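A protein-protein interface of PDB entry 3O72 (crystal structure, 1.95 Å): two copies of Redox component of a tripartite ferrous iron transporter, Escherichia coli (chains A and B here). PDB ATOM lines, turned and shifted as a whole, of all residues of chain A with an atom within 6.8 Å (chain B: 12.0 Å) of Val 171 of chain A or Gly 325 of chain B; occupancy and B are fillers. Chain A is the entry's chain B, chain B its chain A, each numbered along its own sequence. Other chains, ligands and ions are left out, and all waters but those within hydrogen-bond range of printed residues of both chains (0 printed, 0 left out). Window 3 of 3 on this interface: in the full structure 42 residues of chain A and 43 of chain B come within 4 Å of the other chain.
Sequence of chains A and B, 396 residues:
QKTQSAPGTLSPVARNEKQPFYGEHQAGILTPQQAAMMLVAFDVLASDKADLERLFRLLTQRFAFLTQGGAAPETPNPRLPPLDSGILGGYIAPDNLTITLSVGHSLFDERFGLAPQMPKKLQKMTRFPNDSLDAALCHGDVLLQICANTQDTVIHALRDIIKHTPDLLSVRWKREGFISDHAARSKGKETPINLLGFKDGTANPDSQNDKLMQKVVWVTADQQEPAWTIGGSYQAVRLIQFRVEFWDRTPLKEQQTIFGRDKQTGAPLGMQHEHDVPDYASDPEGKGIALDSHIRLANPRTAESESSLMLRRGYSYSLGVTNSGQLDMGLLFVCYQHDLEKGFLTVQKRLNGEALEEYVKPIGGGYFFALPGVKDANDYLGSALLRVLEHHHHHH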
ATOM      1  N   VAL A  40     -12.902  14.601  -5.989  1.00  0.00           N
ATOM      2  CA  VAL A  40     -13.638  13.391  -5.681  1.00  0.00           C
ATOM      3  C   VAL A  40     -14.998  13.776  -5.102  1.00  0.00           C
ATOM      4  O   VAL A  40     -15.090  14.457  -4.079  1.00  0.00           O
ATOM      5  CB  VAL A  40     -12.830  12.439  -4.766  1.00  0.00           C
ATOM      6  CG1 VAL A  40     -12.291  13.192  -3.548  1.00  0.00           C
ATOM      7  CG2 VAL A  40     -13.690  11.237  -4.334  1.00  0.00           C
ATOM      8  N   ALA A  41     -16.051  13.379  -5.805  1.00  0.00           N
ATOM      9  CA  ALA A  41     -17.421  13.630  -5.369  1.00  0.00           C
ATOM     10  C   ALA A  41     -17.945  12.430  -4.591  1.00  0.00           C
ATOM     11  O   ALA A  41     -17.642  11.296  -4.932  1.00  0.00           O
ATOM     12  CB  ALA A  41     -18.304  13.917  -6.577  1.00  0.00           C
ATOM     13  N   PHE A  42     -18.722  12.683  -3.542  1.00  0.00           N
ATOM     14  CA  PHE A  42     -19.309  11.609  -2.756  1.00  0.00           C
ATOM     15  C   PHE A  42     -20.834  11.732  -2.687  1.00  0.00           C
ATOM     16  O   PHE A  42     -21.389  12.835  -2.737  1.00  0.00           O
ATOM     17  CB  PHE A  42     -18.796  11.625  -1.314  1.00  0.00           C
ATOM     18  CG  PHE A  42     -17.299  11.426  -1.169  1.00  0.00           C
ATOM     19  CD1 PHE A  42     -16.775  10.169  -0.906  1.00  0.00           C
ATOM     20  CD2 PHE A  42     -16.425  12.507  -1.253  1.00  0.00           C
ATOM     21  CE1 PHE A  42     -15.399   9.985  -0.725  1.00  0.00           C
ATOM     22  CE2 PHE A  42     -15.043  12.326  -1.075  1.00  0.00           C
ATOM     23  CZ  PHE A  42     -14.535  11.069  -0.825  1.00  0.00           C
ATOM     24  N   ASP A  43     -21.489  10.584  -2.575  1.00  0.00           N
ATOM     25  CA  ASP A  43     -22.852  10.510  -2.049  1.00  0.00           C
ATOM     26  C   ASP A  43     -22.760  10.489  -0.516  1.00  0.00           C
ATOM     27  O   ASP A  43     -21.939   9.762   0.051  1.00  0.00           O
ATOM     28  CB  ASP A  43     -23.520   9.221  -2.531  1.00  0.00           C
ATOM     29  CG  ASP A  43     -23.523   9.096  -4.046  1.00  0.00           C
ATOM     30  OD1 ASP A  43     -23.967  10.048  -4.708  1.00  0.00           O
ATOM     31  OD2 ASP A  43     -23.080   8.052  -4.580  1.00  0.00           O
ATOM     32  N   LEU A 158      -7.192  10.656   0.433  1.00  0.00           N
ATOM     33  CA  LEU A 158      -8.439   9.992   0.052  1.00  0.00           C
ATOM     34  C   LEU A 158      -8.663   8.675   0.830  1.00  0.00           C
ATOM     35  O   LEU A 158      -9.736   8.459   1.377  1.00  0.00           O
ATOM     36  CB  LEU A 158      -8.483   9.744  -1.465  1.00  0.00           C
ATOM     37  CG  LEU A 158      -9.684   8.929  -1.965  1.00  0.00           C
ATOM     38  CD1 LEU A 158     -11.006   9.628  -1.617  1.00  0.00           C
ATOM     39  CD2 LEU A 158      -9.565   8.685  -3.461  1.00  0.00           C
ATOM     40  N   ILE A 162     -11.750   7.829   3.358  1.00  0.00           N
ATOM     41  CA  ILE A 162     -12.599   6.665   3.113  1.00  0.00           C
ATOM     42  C   ILE A 162     -12.606   5.700   4.302  1.00  0.00           C
ATOM     43  O   ILE A 162     -13.659   5.184   4.699  1.00  0.00           O
ATOM     44  CB  ILE A 162     -12.160   5.903   1.857  1.00  0.00           C
ATOM     45  CG1 ILE A 162     -12.512   6.698   0.605  1.00  0.00           C
ATOM     46  CG2 ILE A 162     -12.844   4.534   1.784  1.00  0.00           C
ATOM     47  CD1 ILE A 162     -12.035   6.028  -0.673  1.00  0.00           C
ATOM     48  N   LEU A 169     -19.886   7.948   3.741  1.00  0.00           N
ATOM     49  CA  LEU A 169     -19.540   8.410   2.405  1.00  0.00           C
ATOM     50  C   LEU A 169     -19.426   7.262   1.413  1.00  0.00           C
ATOM     51  O   LEU A 169     -18.926   6.177   1.739  1.00  0.00           O
ATOM     52  CB  LEU A 169     -18.228   9.206   2.426  1.00  0.00           C
ATOM     53  CG  LEU A 169     -18.252  10.561   3.135  1.00  0.00           C
ATOM     54  CD1 LEU A 169     -16.878  11.193   3.063  1.00  0.00           C
ATOM     55  CD2 LEU A 169     -19.279  11.505   2.501  1.00  0.00           C
ATOM     56  N   SER A 170     -19.883   7.527   0.194  1.00  0.00           N
ATOM     57  CA  SER A 170     -19.704   6.617  -0.923  1.00  0.00           C
ATOM     58  C   SER A 170     -19.117   7.396  -2.102  1.00  0.00           C
ATOM     59  O   SER A 170     -19.683   8.409  -2.513  1.00  0.00           O
ATOM     60  CB  SER A 170     -21.064   6.025  -1.321  1.00  0.00           C
ATOM     61  OG  SER A 170     -20.937   5.190  -2.451  1.00  0.00           O
ATOM     62  N   VAL A 171     -18.005   6.925  -2.665  1.00  0.00           N
ATOM     63  CA  VAL A 171     -17.393   7.638  -3.788  1.00  0.00           C
ATOM     64  C   VAL A 171     -18.291   7.590  -5.022  1.00  0.00           C
ATOM     65  O   VAL A 171     -18.703   6.526  -5.453  1.00  0.00           O
ATOM     66  CB  VAL A 171     -15.992   7.106  -4.153  1.00  0.00           C
ATOM     67  CG1 VAL A 171     -15.453   7.838  -5.382  1.00  0.00           C
ATOM     68  CG2 VAL A 171     -15.052   7.275  -2.992  1.00  0.00           C
ATOM     69  N   ARG A 172     -18.585   8.753  -5.586  1.00  0.00           N
ATOM     70  CA  ARG A 172     -19.491   8.834  -6.716  1.00  0.00           C
ATOM     71  C   ARG A 172     -18.708   8.933  -8.024  1.00  0.00           C
ATOM     72  O   ARG A 172     -18.974   8.193  -8.983  1.00  0.00           O
ATOM     73  CB  ARG A 172     -20.383  10.051  -6.545  1.00  0.00           C
ATOM     74  CG  ARG A 172     -21.374  10.244  -7.648  1.00  0.00           C
ATOM     75  CD  ARG A 172     -22.192  11.459  -7.345  1.00  0.00           C
ATOM     76  NE  ARG A 172     -23.170  11.698  -8.392  1.00  0.00           N
ATOM     77  CZ  ARG A 172     -24.370  11.134  -8.422  1.00  0.00           C
ATOM     78  NH1 ARG A 172     -24.727  10.285  -7.458  1.00  0.00           N
ATOM     79  NH2 ARG A 172     -25.207  11.420  -9.418  1.00  0.00           N
ATOM     80  N   TRP A 173     -17.748   9.856  -8.063  1.00  0.00           N
ATOM     81  CA  TRP A 173     -16.823   9.961  -9.182  1.00  0.00           C
ATOM     82  C   TRP A 173     -15.506  10.584  -8.705  1.00  0.00           C
ATOM     83  O   TRP A 173     -15.467  11.243  -7.662  1.00  0.00           O
ATOM     84  CB  TRP A 173     -17.424  10.705 -10.396  1.00  0.00           C
ATOM     85  CG  TRP A 173     -17.906  12.144 -10.167  1.00  0.00           C
ATOM     86  CD1 TRP A 173     -19.192  12.555  -9.941  1.00  0.00           C
ATOM     87  CD2 TRP A 173     -17.105  13.339 -10.210  1.00  0.00           C
ATOM     88  NE1 TRP A 173     -19.238  13.931  -9.822  1.00  0.00           N
ATOM     89  CE2 TRP A 173     -17.971  14.433  -9.970  1.00  0.00           C
ATOM     90  CE3 TRP A 173     -15.744  13.586 -10.404  1.00  0.00           C
ATOM     91  CZ2 TRP A 173     -17.514  15.762  -9.932  1.00  0.00           C
ATOM     92  CZ3 TRP A 173     -15.289  14.905 -10.365  1.00  0.00           C
ATOM     93  CH2 TRP A 173     -16.176  15.975 -10.125  1.00  0.00           C
ATOM     94  N   LYS A 174     -14.435  10.328  -9.450  1.00  0.00           N
ATOM     95  CA  LYS A 174     -13.096  10.770  -9.066  1.00  0.00           C
ATOM     96  C   LYS A 174     -12.253  11.028 -10.289  1.00  0.00           C
ATOM     97  O   LYS A 174     -12.218  10.224 -11.211  1.00  0.00           O
ATOM     98  CB  LYS A 174     -12.394   9.713  -8.190  1.00  0.00           C
ATOM     99  CG  LYS A 174     -10.867   9.947  -8.024  1.00  0.00           C
ATOM    100  CD  LYS A 174     -10.225   8.955  -7.049  1.00  0.00           C
ATOM    101  CE  LYS A 174      -9.350   7.923  -7.730  1.00  0.00           C
ATOM    102  NZ  LYS A 174      -8.257   8.500  -8.564  1.00  0.00           N
ATOM    103  N   GLN B 241      -5.277  -4.579 -11.523  1.00  0.00           N
ATOM    104  CA  GLN B 241      -6.152  -3.776 -10.687  1.00  0.00           C
ATOM    105  C   GLN B 241      -6.234  -4.317  -9.254  1.00  0.00           C
ATOM    106  O   GLN B 241      -6.233  -5.537  -9.045  1.00  0.00           O
ATOM    107  CB  GLN B 241      -7.527  -3.768 -11.351  1.00  0.00           C
ATOM    108  CG  GLN B 241      -8.577  -2.910 -10.723  1.00  0.00           C
ATOM    109  CD  GLN B 241      -9.853  -2.930 -11.562  1.00  0.00           C
ATOM    110  OE1 GLN B 241     -10.879  -3.441 -11.123  1.00  0.00           O
ATOM    111  NE2 GLN B 241      -9.775  -2.410 -12.791  1.00  0.00           N
ATOM    112  N   PHE B 242      -6.294  -3.414  -8.271  1.00  0.00           N
ATOM    113  CA  PHE B 242      -6.374  -3.795  -6.853  1.00  0.00           C
ATOM    114  C   PHE B 242      -7.793  -3.622  -6.304  1.00  0.00           C
ATOM    115  O   PHE B 242      -8.500  -2.700  -6.693  1.00  0.00           O
ATOM    116  CB  PHE B 242      -5.472  -2.923  -5.968  1.00  0.00           C
ATOM    117  CG  PHE B 242      -4.015  -3.043  -6.241  1.00  0.00           C
ATOM    118  CD1 PHE B 242      -3.515  -4.084  -7.011  1.00  0.00           C
ATOM    119  CD2 PHE B 242      -3.131  -2.095  -5.710  1.00  0.00           C
ATOM    120  CE1 PHE B 242      -2.151  -4.185  -7.253  1.00  0.00           C
ATOM    121  CE2 PHE B 242      -1.769  -2.191  -5.930  1.00  0.00           C
ATOM    122  CZ  PHE B 242      -1.272  -3.224  -6.708  1.00  0.00           C
ATOM    123  N   ARG B 243      -8.211  -4.506  -5.400  1.00  0.00           N
ATOM    124  CA  ARG B 243      -9.464  -4.303  -4.685  1.00  0.00           C
ATOM    125  C   ARG B 243      -9.089  -3.510  -3.434  1.00  0.00           C
ATOM    126  O   ARG B 243      -8.856  -4.063  -2.362  1.00  0.00           O
ATOM    127  CB  ARG B 243     -10.154  -5.639  -4.372  1.00  0.00           C
ATOM    128  CG  ARG B 243     -10.744  -6.297  -5.634  1.00  0.00           C
ATOM    129  CD  ARG B 243     -11.447  -7.612  -5.332  1.00  0.00           C
ATOM    130  NE  ARG B 243     -12.576  -7.459  -4.410  1.00  0.00           N
ATOM    131  CZ  ARG B 243     -13.165  -8.484  -3.797  1.00  0.00           C
ATOM    132  NH1 ARG B 243     -12.709  -9.721  -4.001  1.00  0.00           N
ATOM    133  NH2 ARG B 243     -14.191  -8.279  -2.971  1.00  0.00           N
ATOM    134  N   VAL B 244      -8.971  -2.196  -3.614  1.00  0.00           N
ATOM    135  CA  VAL B 244      -8.386  -1.335  -2.597  1.00  0.00           C
ATOM    136  C   VAL B 244      -9.155  -1.324  -1.284  1.00  0.00           C
ATOM    137  O   VAL B 244      -8.573  -1.558  -0.227  1.00  0.00           O
ATOM    138  CB  VAL B 244      -8.226   0.112  -3.106  1.00  0.00           C
ATOM    139  CG1 VAL B 244      -7.487   0.931  -2.071  1.00  0.00           C
ATOM    140  CG2 VAL B 244      -7.479   0.113  -4.420  1.00  0.00           C
ATOM    141  N   GLU B 245     -10.456  -1.043  -1.347  1.00  0.00           N
ATOM    142  CA  GLU B 245     -11.264  -0.940  -0.126  1.00  0.00           C
ATOM    143  C   GLU B 245     -11.277  -2.262   0.626  1.00  0.00           C
ATOM    144  O   GLU B 245     -11.163  -2.294   1.848  1.00  0.00           O
ATOM    145  CB  GLU B 245     -12.701  -0.478  -0.441  1.00  0.00           C
ATOM    146  CG  GLU B 245     -12.790   0.919  -1.083  1.00  0.00           C
ATOM    147  CD  GLU B 245     -12.753   0.893  -2.614  1.00  0.00           C
ATOM    148  OE1 GLU B 245     -12.392  -0.157  -3.201  1.00  0.00           O
ATOM    149  OE2 GLU B 245     -13.073   1.931  -3.234  1.00  0.00           O
ATOM    150  N   PHE B 246     -11.424  -3.353  -0.116  1.00  0.00           N
ATOM    151  CA  PHE B 246     -11.383  -4.697   0.447  1.00  0.00           C
ATOM    152  C   PHE B 246     -10.046  -4.929   1.163  1.00  0.00           C
ATOM    153  O   PHE B 246     -10.002  -5.400   2.304  1.00  0.00           O
ATOM    154  CB  PHE B 246     -11.583  -5.714  -0.681  1.00  0.00           C
ATOM    155  CG  PHE B 246     -11.611  -7.139  -0.227  1.00  0.00           C
ATOM    156  CD1 PHE B 246     -12.075  -7.477   1.030  1.00  0.00           C
ATOM    157  CD2 PHE B 246     -11.179  -8.143  -1.069  1.00  0.00           C
ATOM    158  CE1 PHE B 246     -12.103  -8.805   1.439  1.00  0.00           C
ATOM    159  CE2 PHE B 246     -11.203  -9.455  -0.670  1.00  0.00           C
ATOM    160  CZ  PHE B 246     -11.676  -9.792   0.581  1.00  0.00           C
ATOM    161  N   ASP B 248      -7.931  -2.610   2.333  1.00  0.00           N
ATOM    162  CA  ASP B 248      -7.804  -1.704   3.481  1.00  0.00           C
ATOM    163  C   ASP B 248      -8.590  -2.131   4.738  1.00  0.00           C
ATOM    164  O   ASP B 248      -8.285  -1.686   5.853  1.00  0.00           O
ATOM    165  CB  ASP B 248      -8.178  -0.260   3.086  1.00  0.00           C
ATOM    166  CG  ASP B 248      -7.040   0.467   2.333  1.00  0.00           C
ATOM    167  OD1 ASP B 248      -5.903  -0.047   2.289  1.00  0.00           O
ATOM    168  OD2 ASP B 248      -7.292   1.560   1.782  1.00  0.00           O
ATOM    169  N   ARG B 249      -9.614  -2.954   4.554  1.00  0.00           N
ATOM    170  CA  ARG B 249     -10.396  -3.458   5.681  1.00  0.00           C
ATOM    171  C   ARG B 249      -9.936  -4.861   6.073  1.00  0.00           C
ATOM    172  O   ARG B 249     -10.539  -5.510   6.921  1.00  0.00           O
ATOM    173  CB  ARG B 249     -11.899  -3.443   5.354  1.00  0.00           C
ATOM    174  CG  ARG B 249     -12.411  -4.627   4.558  1.00  0.00           C
ATOM    175  CD  ARG B 249     -13.955  -4.598   4.446  1.00  0.00           C
ATOM    176  NE  ARG B 249     -14.489  -5.563   3.479  1.00  0.00           N
ATOM    177  CZ  ARG B 249     -14.878  -5.252   2.237  1.00  0.00           C
ATOM    178  NH1 ARG B 249     -14.803  -3.993   1.790  1.00  0.00           N
ATOM    179  NH2 ARG B 249     -15.347  -6.201   1.435  1.00  0.00           N
ATOM    180  N   SER B 318      -3.296   5.002 -10.801  1.00  0.00           N
ATOM    181  CA  SER B 318      -4.541   5.422 -10.170  1.00  0.00           C
ATOM    182  C   SER B 318      -5.387   6.139 -11.223  1.00  0.00           C
ATOM    183  O   SER B 318      -4.918   7.084 -11.852  1.00  0.00           O
ATOM    184  CB  SER B 318      -4.226   6.334  -8.982  1.00  0.00           C
ATOM    185  OG  SER B 318      -5.410   6.777  -8.345  1.00  0.00           O
ATOM    186  N   LEU B 319      -6.612   5.670 -11.453  1.00  0.00           N
ATOM    187  CA  LEU B 319      -7.463   6.254 -12.496  1.00  0.00           C
ATOM    188  C   LEU B 319      -8.688   6.932 -11.883  1.00  0.00           C
ATOM    189  O   LEU B 319      -8.569   7.884 -11.104  1.00  0.00           O
ATOM    190  CB  LEU B 319      -7.892   5.186 -13.507  1.00  0.00           C
ATOM    191  CG  LEU B 319      -6.742   4.343 -14.064  1.00  0.00           C
ATOM    192  CD1 LEU B 319      -7.199   3.457 -15.211  1.00  0.00           C
ATOM    193  CD2 LEU B 319      -5.602   5.266 -14.519  1.00  0.00           C
ATOM    194  N   GLY B 320      -9.864   6.435 -12.229  1.00  0.00           N
ATOM    195  CA  GLY B 320     -11.095   6.907 -11.627  1.00  0.00           C
ATOM    196  C   GLY B 320     -11.695   5.832 -10.730  1.00  0.00           C
ATOM    197  O   GLY B 320     -11.076   5.409  -9.759  1.00  0.00           O
ATOM    198  N   VAL B 321     -12.908   5.398 -11.047  1.00  0.00           N
ATOM    199  CA  VAL B 321     -13.561   4.338 -10.291  1.00  0.00           C
ATOM    200  C   VAL B 321     -13.851   3.153 -11.206  1.00  0.00           C
ATOM    201  O   VAL B 321     -13.806   3.281 -12.431  1.00  0.00           O
ATOM    202  CB  VAL B 321     -14.865   4.831  -9.634  1.00  0.00           C
ATOM    203  CG1 VAL B 321     -14.570   5.968  -8.676  1.00  0.00           C
ATOM    204  CG2 VAL B 321     -15.879   5.261 -10.702  1.00  0.00           C
ATOM    205  N   THR B 322     -14.130   1.995 -10.616  1.00  0.00           N
ATOM    206  CA  THR B 322     -14.447   0.816 -11.405  1.00  0.00           C
ATOM    207  C   THR B 322     -15.945   0.856 -11.737  1.00  0.00           C
ATOM    208  O   THR B 322     -16.631   1.822 -11.409  1.00  0.00           O
ATOM    209  CB  THR B 322     -14.140  -0.477 -10.626  1.00  0.00           C
ATOM    210  OG1 THR B 322     -14.937  -0.517  -9.434  1.00  0.00           O
ATOM    211  CG2 THR B 322     -12.649  -0.535 -10.240  1.00  0.00           C
ATOM    212  N   ASN B 323     -16.467  -0.193 -12.358  1.00  0.00           N
ATOM    213  CA  ASN B 323     -17.912  -0.237 -12.628  1.00  0.00           C
ATOM    214  C   ASN B 323     -18.752  -0.443 -11.365  1.00  0.00           C
ATOM    215  O   ASN B 323     -19.970  -0.269 -11.398  1.00  0.00           O
ATOM    216  CB  ASN B 323     -18.245  -1.324 -13.636  1.00  0.00           C
ATOM    217  CG  ASN B 323     -17.964  -2.695 -13.099  1.00  0.00           C
ATOM    218  OD1 ASN B 323     -16.946  -2.914 -12.435  1.00  0.00           O
ATOM    219  ND2 ASN B 323     -18.873  -3.636 -13.357  1.00  0.00           N
ATOM    220  N   SER B 324     -18.114  -0.823 -10.258  1.00  0.00           N
ATOM    221  CA  SER B 324     -18.824  -0.925  -8.980  1.00  0.00           C
ATOM    222  C   SER B 324     -18.622   0.311  -8.103  1.00  0.00           C
ATOM    223  O   SER B 324     -18.937   0.296  -6.909  1.00  0.00           O
ATOM    224  CB  SER B 324     -18.417  -2.180  -8.205  1.00  0.00           C
ATOM    225  OG  SER B 324     -17.060  -2.120  -7.805  1.00  0.00           O
ATOM    226  N   GLY B 325     -18.085   1.372  -8.692  1.00  0.00           N
ATOM    227  CA  GLY B 325     -17.883   2.606  -7.958  1.00  0.00           C
ATOM    228  C   GLY B 325     -16.798   2.482  -6.906  1.00  0.00           C
ATOM    229  O   GLY B 325     -16.757   3.247  -5.943  1.00  0.00           O
ATOM    230  N   GLN B 326     -15.912   1.513  -7.089  1.00  0.00           N
ATOM    231  CA  GLN B 326     -14.778   1.384  -6.186  1.00  0.00           C
ATOM    232  C   GLN B 326     -13.519   1.955  -6.813  1.00  0.00           C
ATOM    233  O   GLN B 326     -13.475   2.207  -8.014  1.00  0.00           O
ATOM    234  CB  GLN B 326     -14.638  -0.061  -5.723  1.00  0.00           C
ATOM    235  CG  GLN B 326     -15.871  -0.435  -4.893  1.00  0.00           C
ATOM    236  CD  GLN B 326     -15.848  -1.840  -4.403  1.00  0.00           C
ATOM    237  OE1 GLN B 326     -16.160  -2.778  -5.149  1.00  0.00           O
ATOM    238  NE2 GLN B 326     -15.487  -2.012  -3.134  1.00  0.00           N
ATOM    239  N   LEU B 327     -12.497   2.197  -6.002  1.00  0.00           N
ATOM    240  CA  LEU B 327     -11.351   2.932  -6.514  1.00  0.00           C
ATOM    241  C   LEU B 327     -10.613   2.119  -7.575  1.00  0.00           C
ATOM    242  O   LEU B 327     -10.345   0.941  -7.376  1.00  0.00           O
ATOM    243  CB  LEU B 327     -10.415   3.340  -5.370  1.00  0.00           C
ATOM    244  CG  LEU B 327     -10.980   4.327  -4.342  1.00  0.00           C
ATOM    245  CD1 LEU B 327      -9.977   4.539  -3.214  1.00  0.00           C
ATOM    246  CD2 LEU B 327     -11.359   5.643  -5.005  1.00  0.00           C
ATOM    247  N   ASP B 328     -10.291   2.746  -8.702  1.00  0.00           N
ATOM    248  CA  ASP B 328      -9.488   2.080  -9.730  1.00  0.00           C
ATOM    249  C   ASP B 328      -7.999   2.407  -9.576  1.00  0.00           C
ATOM    250  O   ASP B 328      -7.537   3.453 -10.033  1.00  0.00           O
ATOM    251  CB  ASP B 328      -9.937   2.473 -11.136  1.00  0.00           C
ATOM    252  CG  ASP B 328      -9.329   1.588 -12.209  1.00  0.00           C
ATOM    253  OD1 ASP B 328      -8.443   0.774 -11.887  1.00  0.00           O
ATOM    254  OD2 ASP B 328      -9.740   1.695 -13.381  1.00  0.00           O
ATOM    255  N   MET B 329      -7.259   1.504  -8.946  1.00  0.00           N
ATOM    256  CA  MET B 329      -5.836   1.719  -8.699  1.00  0.00           C
ATOM    257  C   MET B 329      -5.165   0.384  -8.828  1.00  0.00           C
ATOM    258  O   MET B 329      -5.822  -0.650  -8.669  1.00  0.00           O
ATOM    259  CB  MET B 329      -5.601   2.195  -7.267  1.00  0.00           C
ATOM    260  CG  MET B 329      -6.253   3.479  -6.938  1.00  0.00           C
ATOM    261  SD  MET B 329      -5.901   3.902  -5.078  1.00  0.00           S
ATOM    262  CE  MET B 329      -6.694   5.693  -5.142  1.00  0.00           C
ATOM    263  N   LYS B 361      -6.715  -8.159  -9.893  1.00  0.00           N
ATOM    264  CA  LYS B 361      -7.419  -8.511 -11.110  1.00  0.00           C
ATOM    265  C   LYS B 361      -6.578  -8.128 -12.323  1.00  0.00           C
ATOM    266  O   LYS B 361      -6.516  -6.954 -12.682  1.00  0.00           O
ATOM    267  CB  LYS B 361      -8.795  -7.822 -11.115  1.00  0.00           C
ATOM    268  CG  LYS B 361      -9.630  -8.008 -12.379  1.00  0.00           C
ATOM    269  CD  LYS B 361     -10.974  -7.213 -12.250  1.00  0.00           C
ATOM    270  CE  LYS B 361     -11.855  -7.322 -13.495  1.00  0.00           C
ATOM    271  NZ  LYS B 361     -13.152  -6.561 -13.355  1.00  0.00           N
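Of the 12 printed residues of chain A, 4 touch a printed residue of chain B. Of the 21 printed residues of chain B, 6 touch a printed residue of chain A. Hydrophobic or aromatic side chains of chain B within 4 Å of the printed part of chain A: Val 321 and Leu 327. Along chain B the printed residues that touch a printed residue of chain A span positions 318 to 327. Among the printed residues, 7 pairs touch across the chains.
Leu 158 of chain A touches Leu 327 of chain B. Leu 327 of chain B touches Ile 162 of chain A. CG1 of Val 171 of chain A touches CG1 of Val 321 of chain B (3.9 Å). Gly 325 of chain B touches Val 171 of chain A (O to O, 3.8 Å). Gly 320 of chain B touches Lys 174 of chain A (CA to O, 3.5 Å).
The side-chain amino group (NZ) of Lys 174 of chain A is in hydrogen-bond range of the backbone carbonyl oxygen (O) of Leu 319 of chain B (2.6 Å). The side-chain hydroxyl of Ser 318 of chain B sits at hydrogen-bond distance from the side-chain amino group of Lys 174 of chain A (3.3 Å).
No position is printed for both chains.
The backbone NH of Leu 319 of chain B sits at hydrogen-bond distance from the backbone carbonyl oxygen of Asp 328 of chain B. N of Leu 327 of chain B lies within hydrogen-bond range of OE2 of Glu 245 of chain B (2.8 Å). O of Gly 320 of chain B is in hydrogen-bond range of N of Asp 328 of chain B.
Of chain B, only Val 321 and Gly 325 come within 4 Å of Val 171 of chain A. Of chain A, only Val 171 comes within 4 Å of Gly 325 of chain B. No residue of chain B comes within 4 Å of Phe 42 of chain A. No residue of chain B comes within 4 Å of Asp 43 of chain A. Leu 169 of chain A touches none of the printed residues of chain B. Lys 174 of chain A touches three residues of chain B. Of the printed residues of chain A, Val 321 of chain B touches Val 171 (3.9 Å). Of the printed residues of chain B, Ile 162 of chain A touches Leu 327 (3.6 Å). Of the printed residues of chain B, Leu 158 of chain A touches Leu 327 (3.9 Å). Printed residues of chain A within 4 Å of Leu 327 of chain B: Leu 158 (3.9 Å) and Ile 162 (3.6 Å). Of the printed residues of chain A, Ser 318 of chain B touches Lys 174. Asp 248 of chain B touches none of the printed residues of chain A. Lys 361 of chain B touches none of the printed residues of chain A. The nearest printed residue of chain A that does not touch Gly 325 of chain B is Ser 170 of chain A (5.8 Å).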
